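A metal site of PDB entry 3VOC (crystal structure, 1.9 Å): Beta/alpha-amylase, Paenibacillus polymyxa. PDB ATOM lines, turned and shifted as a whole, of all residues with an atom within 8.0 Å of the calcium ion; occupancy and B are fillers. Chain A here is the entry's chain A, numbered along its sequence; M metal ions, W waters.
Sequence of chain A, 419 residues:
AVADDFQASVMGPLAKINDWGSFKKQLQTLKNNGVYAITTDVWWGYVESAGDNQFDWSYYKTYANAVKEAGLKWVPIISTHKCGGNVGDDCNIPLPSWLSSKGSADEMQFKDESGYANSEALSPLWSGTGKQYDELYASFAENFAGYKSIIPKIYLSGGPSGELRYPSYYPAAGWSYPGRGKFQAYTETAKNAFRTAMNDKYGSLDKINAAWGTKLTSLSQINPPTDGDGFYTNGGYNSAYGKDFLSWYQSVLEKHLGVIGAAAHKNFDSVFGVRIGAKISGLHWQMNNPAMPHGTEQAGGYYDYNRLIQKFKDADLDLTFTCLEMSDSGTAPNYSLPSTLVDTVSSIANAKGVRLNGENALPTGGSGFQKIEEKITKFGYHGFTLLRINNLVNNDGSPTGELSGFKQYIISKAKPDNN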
ATOM      1  N   TRP A  44     -32.277  -6.021 -14.948  1.00  0.00           N
ATOM      2  CA  TRP A  44     -31.479  -7.250 -14.950  1.00  0.00           C
ATOM      3  C   TRP A  44     -30.039  -6.980 -15.386  1.00  0.00           C
ATOM      4  O   TRP A  44     -29.079  -7.501 -14.782  1.00  0.00           O
ATOM      5  CB  TRP A  44     -32.126  -8.295 -15.849  1.00  0.00           C
ATOM      6  CG  TRP A  44     -31.670  -9.708 -15.557  1.00  0.00           C
ATOM      7  CD1 TRP A  44     -30.877 -10.143 -14.502  1.00  0.00           C
ATOM      8  CD2 TRP A  44     -32.019 -10.893 -16.292  1.00  0.00           C
ATOM      9  NE1 TRP A  44     -30.710 -11.509 -14.566  1.00  0.00           N
ATOM     10  CE2 TRP A  44     -31.396 -11.990 -15.654  1.00  0.00           C
ATOM     11  CE3 TRP A  44     -32.795 -11.121 -17.451  1.00  0.00           C
ATOM     12  CZ2 TRP A  44     -31.523 -13.295 -16.131  1.00  0.00           C
ATOM     13  CZ3 TRP A  44     -32.943 -12.419 -17.903  1.00  0.00           C
ATOM     14  CH2 TRP A  44     -32.302 -13.492 -17.245  1.00  0.00           C
ATOM     15  N   GLU A  48     -27.061  -8.391 -12.692  1.00  0.00           N
ATOM     16  CA  GLU A  48     -26.422  -9.688 -12.940  1.00  0.00           C
ATOM     17  C   GLU A  48     -25.607  -9.611 -14.235  1.00  0.00           C
ATOM     18  O   GLU A  48     -25.676 -10.496 -15.081  1.00  0.00           O
ATOM     19  CB  GLU A  48     -27.480 -10.809 -12.979  1.00  0.00           C
ATOM     20  CG  GLU A  48     -26.939 -12.239 -12.779  1.00  0.00           C
ATOM     21  CD  GLU A  48     -28.013 -13.321 -12.876  1.00  0.00           C
ATOM     22  OE1 GLU A  48     -29.236 -12.998 -12.816  1.00  0.00           O
ATOM     23  OE2 GLU A  48     -27.646 -14.509 -12.995  1.00  0.00           O
ATOM     24  N   GLY A  51     -21.749 -12.065 -14.815  1.00  0.00           N
ATOM     25  CA  GLY A  51     -21.758 -13.506 -15.041  1.00  0.00           C
ATOM     26  C   GLY A  51     -22.987 -14.128 -14.418  1.00  0.00           C
ATOM     27  O   GLY A  51     -23.645 -13.493 -13.581  1.00  0.00           O
ATOM     28  N   ASP A  52     -23.315 -15.346 -14.835  1.00  0.00           N
ATOM     29  CA  ASP A  52     -24.473 -16.053 -14.298  1.00  0.00           C
ATOM     30  C   ASP A  52     -24.309 -16.181 -12.795  1.00  0.00           C
ATOM     31  O   ASP A  52     -23.316 -16.719 -12.302  1.00  0.00           O
ATOM     32  CB  ASP A  52     -24.627 -17.435 -14.946  1.00  0.00           C
ATOM     33  CG  ASP A  52     -25.947 -18.111 -14.597  1.00  0.00           C
ATOM     34  OD1 ASP A  52     -26.835 -17.483 -13.972  1.00  0.00           O
ATOM     35  OD2 ASP A  52     -26.115 -19.300 -14.937  1.00  0.00           O
ATOM     36  N   ASN A  53     -25.274 -15.604 -12.073  1.00  0.00           N
ATOM     37  CA  ASN A  53     -25.317 -15.633 -10.609  1.00  0.00           C
ATOM     38  C   ASN A  53     -24.179 -14.871  -9.946  1.00  0.00           C
ATOM     39  O   ASN A  53     -23.809 -15.143  -8.804  1.00  0.00           O
ATOM     40  CB  ASN A  53     -25.436 -17.067 -10.076  1.00  0.00           C
ATOM     41  CG  ASN A  53     -26.702 -17.753 -10.535  1.00  0.00           C
ATOM     42  OD1 ASN A  53     -27.655 -17.094 -10.960  1.00  0.00           O
ATOM     43  ND2 ASN A  53     -26.719 -19.061 -10.456  1.00  0.00           N
ATOM     44  N   GLN A  54     -23.634 -13.913 -10.678  1.00  0.00           N
ATOM     45  CA  GLN A  54     -22.730 -12.941 -10.110  1.00  0.00           C
ATOM     46  C   GLN A  54     -23.486 -11.615 -10.049  1.00  0.00           C
ATOM     47  O   GLN A  54     -23.706 -10.952 -11.068  1.00  0.00           O
ATOM     48  CB  GLN A  54     -21.450 -12.829 -10.949  1.00  0.00           C
ATOM     49  CG  GLN A  54     -20.427 -11.925 -10.320  1.00  0.00           C
ATOM     50  CD  GLN A  54     -19.087 -11.862 -11.079  1.00  0.00           C
ATOM     51  OE1 GLN A  54     -18.755 -12.726 -11.896  1.00  0.00           O
ATOM     52  NE2 GLN A  54     -18.336 -10.809 -10.795  1.00  0.00           N
ATOM     53  N   PHE A  55     -23.895 -11.233  -8.850  1.00  0.00           N
ATOM     54  CA  PHE A  55     -24.819 -10.115  -8.671  1.00  0.00           C
ATOM     55  C   PHE A  55     -24.132  -8.855  -8.182  1.00  0.00           C
ATOM     56  O   PHE A  55     -23.110  -8.925  -7.489  1.00  0.00           O
ATOM     57  CB  PHE A  55     -25.936 -10.523  -7.692  1.00  0.00           C
ATOM     58  CG  PHE A  55     -26.806 -11.619  -8.205  1.00  0.00           C
ATOM     59  CD1 PHE A  55     -27.863 -11.327  -9.098  1.00  0.00           C
ATOM     60  CD2 PHE A  55     -26.585 -12.937  -7.821  1.00  0.00           C
ATOM     61  CE1 PHE A  55     -28.667 -12.353  -9.600  1.00  0.00           C
ATOM     62  CE2 PHE A  55     -27.388 -13.963  -8.323  1.00  0.00           C
ATOM     63  CZ  PHE A  55     -28.428 -13.662  -9.211  1.00  0.00           C
ATOM     64  N   PRO A  96     -28.388  -9.292 -19.536  1.00  0.00           N
ATOM     65  CA  PRO A  96     -27.022  -9.715 -19.229  1.00  0.00           C
ATOM     66  C   PRO A  96     -26.367 -10.404 -20.432  1.00  0.00           C
ATOM     67  O   PRO A  96     -26.936 -11.338 -21.011  1.00  0.00           O
ATOM     68  CB  PRO A  96     -27.235 -10.701 -18.074  1.00  0.00           C
ATOM     69  CG  PRO A  96     -28.438 -10.125 -17.341  1.00  0.00           C
ATOM     70  CD  PRO A  96     -29.343  -9.679 -18.474  1.00  0.00           C
ATOM     71  N   TRP A  98     -23.895 -12.424 -20.962  1.00  0.00           N
ATOM     72  CA  TRP A  98     -23.484 -13.830 -20.879  1.00  0.00           C
ATOM     73  C   TRP A  98     -24.623 -14.798 -21.219  1.00  0.00           C
ATOM     74  O   TRP A  98     -24.373 -15.996 -21.492  1.00  0.00           O
ATOM     75  CB  TRP A  98     -22.897 -14.154 -19.496  1.00  0.00           C
ATOM     76  CG  TRP A  98     -23.775 -13.671 -18.374  1.00  0.00           C
ATOM     77  CD1 TRP A  98     -23.645 -12.509 -17.668  1.00  0.00           C
ATOM     78  CD2 TRP A  98     -24.944 -14.313 -17.871  1.00  0.00           C
ATOM     79  NE1 TRP A  98     -24.655 -12.402 -16.731  1.00  0.00           N
ATOM     80  CE2 TRP A  98     -25.471 -13.498 -16.843  1.00  0.00           C
ATOM     81  CE3 TRP A  98     -25.586 -15.518 -18.174  1.00  0.00           C
ATOM     82  CZ2 TRP A  98     -26.616 -13.837 -16.131  1.00  0.00           C
ATOM     83  CZ3 TRP A  98     -26.740 -15.862 -17.465  1.00  0.00           C
ATOM     84  CH2 TRP A  98     -27.240 -15.019 -16.458  1.00  0.00           C
ATOM     85  N   LEU A  99     -25.868 -14.314 -21.194  1.00  0.00           N
ATOM     86  CA  LEU A  99     -27.019 -15.163 -21.526  1.00  0.00           C
ATOM     87  C   LEU A  99     -26.877 -15.827 -22.900  1.00  0.00           C
ATOM     88  O   LEU A  99     -27.286 -16.961 -23.087  1.00  0.00           O
ATOM     89  CB  LEU A  99     -28.344 -14.388 -21.452  1.00  0.00           C
ATOM     90  CG  LEU A  99     -28.901 -14.157 -20.041  1.00  0.00           C
ATOM     91  CD1 LEU A  99     -29.902 -12.991 -20.011  1.00  0.00           C
ATOM     92  CD2 LEU A  99     -29.578 -15.444 -19.490  1.00  0.00           C
ATOM     93  N   LYS A 102     -25.470 -19.230 -23.056  1.00  0.00           N
ATOM     94  CA  LYS A 102     -26.167 -20.241 -22.243  1.00  0.00           C
ATOM     95  C   LYS A 102     -27.282 -21.025 -22.960  1.00  0.00           C
ATOM     96  O   LYS A 102     -27.776 -22.033 -22.447  1.00  0.00           O
ATOM     97  CB  LYS A 102     -26.714 -19.610 -20.951  1.00  0.00           C
ATOM     98  CG  LYS A 102     -25.639 -19.099 -19.994  1.00  0.00           C
ATOM     99  CD  LYS A 102     -24.805 -20.240 -19.404  1.00  0.00           C
ATOM    100  CE  LYS A 102     -23.959 -19.784 -18.222  1.00  0.00           C
ATOM    101  NZ  LYS A 102     -22.613 -19.269 -18.650  1.00  0.00           N
ATOM    102  N   GLY A 128     -34.498 -22.295 -20.088  1.00  0.00           N
ATOM    103  CA  GLY A 128     -33.753 -21.607 -19.038  1.00  0.00           C
ATOM    104  C   GLY A 128     -34.348 -20.316 -18.479  1.00  0.00           C
ATOM    105  O   GLY A 128     -33.834 -19.783 -17.486  1.00  0.00           O
ATOM    106  N   LYS A 131     -35.823 -20.696 -14.837  1.00  0.00           N
ATOM    107  CA  LYS A 131     -34.712 -20.947 -13.916  1.00  0.00           C
ATOM    108  C   LYS A 131     -33.971 -19.650 -13.644  1.00  0.00           C
ATOM    109  O   LYS A 131     -33.714 -19.319 -12.493  1.00  0.00           O
ATOM    110  CB  LYS A 131     -33.742 -21.995 -14.492  1.00  0.00           C
ATOM    111  CG  LYS A 131     -32.602 -22.350 -13.538  1.00  0.00           C
ATOM    112  CD  LYS A 131     -31.665 -23.421 -14.115  1.00  0.00           C
ATOM    113  CE  LYS A 131     -30.605 -23.788 -13.083  1.00  0.00           C
ATOM    114  NZ  LYS A 131     -29.452 -24.495 -13.720  1.00  0.00           N
ATOM    115  N   GLN A 132     -33.614 -18.924 -14.704  1.00  0.00           N
ATOM    116  CA  GLN A 132     -32.936 -17.626 -14.546  1.00  0.00           C
ATOM    117  C   GLN A 132     -33.733 -16.634 -13.680  1.00  0.00           C
ATOM    118  O   GLN A 132     -33.157 -15.980 -12.810  1.00  0.00           O
ATOM    119  CB  GLN A 132     -32.568 -17.000 -15.893  1.00  0.00           C
ATOM    120  CG  GLN A 132     -31.410 -17.722 -16.618  1.00  0.00           C
ATOM    121  CD  GLN A 132     -30.102 -17.729 -15.828  1.00  0.00           C
ATOM    122  OE1 GLN A 132     -29.779 -16.774 -15.100  1.00  0.00           O
ATOM    123  NE2 GLN A 132     -29.329 -18.792 -16.003  1.00  0.00           N
ATOM    124  N   TYR A 133     -35.042 -16.533 -13.878  1.00  0.00           N
ATOM    125  CA  TYR A 133     -35.845 -15.584 -13.096  1.00  0.00           C
ATOM    126  C   TYR A 133     -35.925 -16.036 -11.643  1.00  0.00           C
ATOM    127  O   TYR A 133     -35.890 -15.228 -10.737  1.00  0.00           O
ATOM    128  CB  TYR A 133     -37.256 -15.420 -13.663  1.00  0.00           C
ATOM    129  CG  TYR A 133     -37.386 -14.650 -14.995  1.00  0.00           C
ATOM    130  CD1 TYR A 133     -36.338 -14.584 -15.913  1.00  0.00           C
ATOM    131  CD2 TYR A 133     -38.595 -14.061 -15.346  1.00  0.00           C
ATOM    132  CE1 TYR A 133     -36.487 -13.899 -17.140  1.00  0.00           C
ATOM    133  CE2 TYR A 133     -38.764 -13.386 -16.563  1.00  0.00           C
ATOM    134  CZ  TYR A 133     -37.706 -13.330 -17.450  1.00  0.00           C
ATOM    135  OH  TYR A 133     -37.879 -12.680 -18.649  1.00  0.00           O
ATOM    136  N   ASP A 134     -36.055 -17.348 -11.457  1.00  0.00           N
ATOM    137  CA  ASP A 134     -36.068 -17.942 -10.103  1.00  0.00           C
ATOM    138  C   ASP A 134     -34.790 -17.558  -9.333  1.00  0.00           C
ATOM    139  O   ASP A 134     -34.867 -17.117  -8.180  1.00  0.00           O
ATOM    140  CB  ASP A 134     -36.257 -19.465 -10.212  1.00  0.00           C
ATOM    141  CG  ASP A 134     -36.497 -20.148  -8.866  1.00  0.00           C
ATOM    142  OD1 ASP A 134     -36.913 -19.500  -7.886  1.00  0.00           O
ATOM    143  OD2 ASP A 134     -36.287 -21.375  -8.816  1.00  0.00           O
ATOM    144  N   GLU A 135     -33.623 -17.720  -9.963  1.00  0.00           N
ATOM    145  CA  GLU A 135     -32.355 -17.319  -9.330  1.00  0.00           C
ATOM    146  C   GLU A 135     -32.309 -15.829  -9.021  1.00  0.00           C
ATOM    147  O   GLU A 135     -31.807 -15.417  -7.974  1.00  0.00           O
ATOM    148  CB  GLU A 135     -31.151 -17.648 -10.218  1.00  0.00           C
ATOM    149  CG  GLU A 135     -30.980 -19.140 -10.536  1.00  0.00           C
ATOM    150  CD  GLU A 135     -29.953 -19.374 -11.632  1.00  0.00           C
ATOM    151  OE1 GLU A 135     -29.809 -18.511 -12.536  1.00  0.00           O
ATOM    152  OE2 GLU A 135     -29.283 -20.420 -11.595  1.00  0.00           O
ATOM    153  N   LEU A 136     -32.807 -15.005  -9.945  1.00  0.00           N
ATOM    154  CA  LEU A 136     -32.771 -13.545  -9.776  1.00  0.00           C
ATOM    155  C   LEU A 136     -33.720 -13.110  -8.643  1.00  0.00           C
ATOM    156  O   LEU A 136     -33.383 -12.225  -7.831  1.00  0.00           O
ATOM    157  CB  LEU A 136     -33.128 -12.849 -11.101  1.00  0.00           C
ATOM    158  CG  LEU A 136     -33.296 -11.321 -11.062  1.00  0.00           C
ATOM    159  CD1 LEU A 136     -31.948 -10.677 -10.735  1.00  0.00           C
ATOM    160  CD2 LEU A 136     -33.824 -10.813 -12.391  1.00  0.00           C
ATOM    161  N   SER A 139     -32.141 -14.077  -5.373  1.00  0.00           N
ATOM    162  CA  SER A 139     -31.101 -13.146  -5.020  1.00  0.00           C
ATOM    163  C   SER A 139     -31.675 -11.823  -4.519  1.00  0.00           C
ATOM    164  O   SER A 139     -31.157 -11.265  -3.545  1.00  0.00           O
ATOM    165  CB  SER A 139     -30.150 -12.887  -6.195  1.00  0.00           C
ATOM    166  OG  SER A 139     -29.048 -12.145  -5.728  1.00  0.00           O
HETATM  167 CA    CA M   1     -28.722 -16.605 -13.039  1.00  0.00          CA
HETATM  168  O   HOH W   1     -30.515 -15.236 -12.426  1.00  0.00           O
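Water W1 lies within hydrogen-bond range of OE1 of Glu 48, O of Gln 132 and N of Leu 136.
The side-chain carboxylate of Glu 48 sits at hydrogen-bond distance from the indole nitrogen of Trp 44, at 2.7 Å.
The indole nitrogen of Trp 98 is in hydrogen-bond range of the backbone carbonyl oxygen of Glu 48 (2.7 Å).
Within 4 Å of the calcium ion: Glu 48, Asp 52, Asn 53, Gln 132 and Glu 135.
The nearest printed residue that does not touch the calcium ion is Trp 98 (4.05 Å).
OE1 of Glu 135 is bound to the calcium ion (2.3 Å).
OD1 of Asp 52 is bound to the calcium ion (2.3 Å).
OE1 of Gln 132 is bound to the calcium ion (2.3 Å).
The calcium ion is bound by water W1, at 2.3 Å.
OE2 of Glu 48 is bound to the calcium ion (2.4 Å).
The side-chain amide oxygen (OD1) of Asn 53 is bound to the calcium ion, 2.4 Å away.
The calcium ion has six donor atoms within binding distance.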
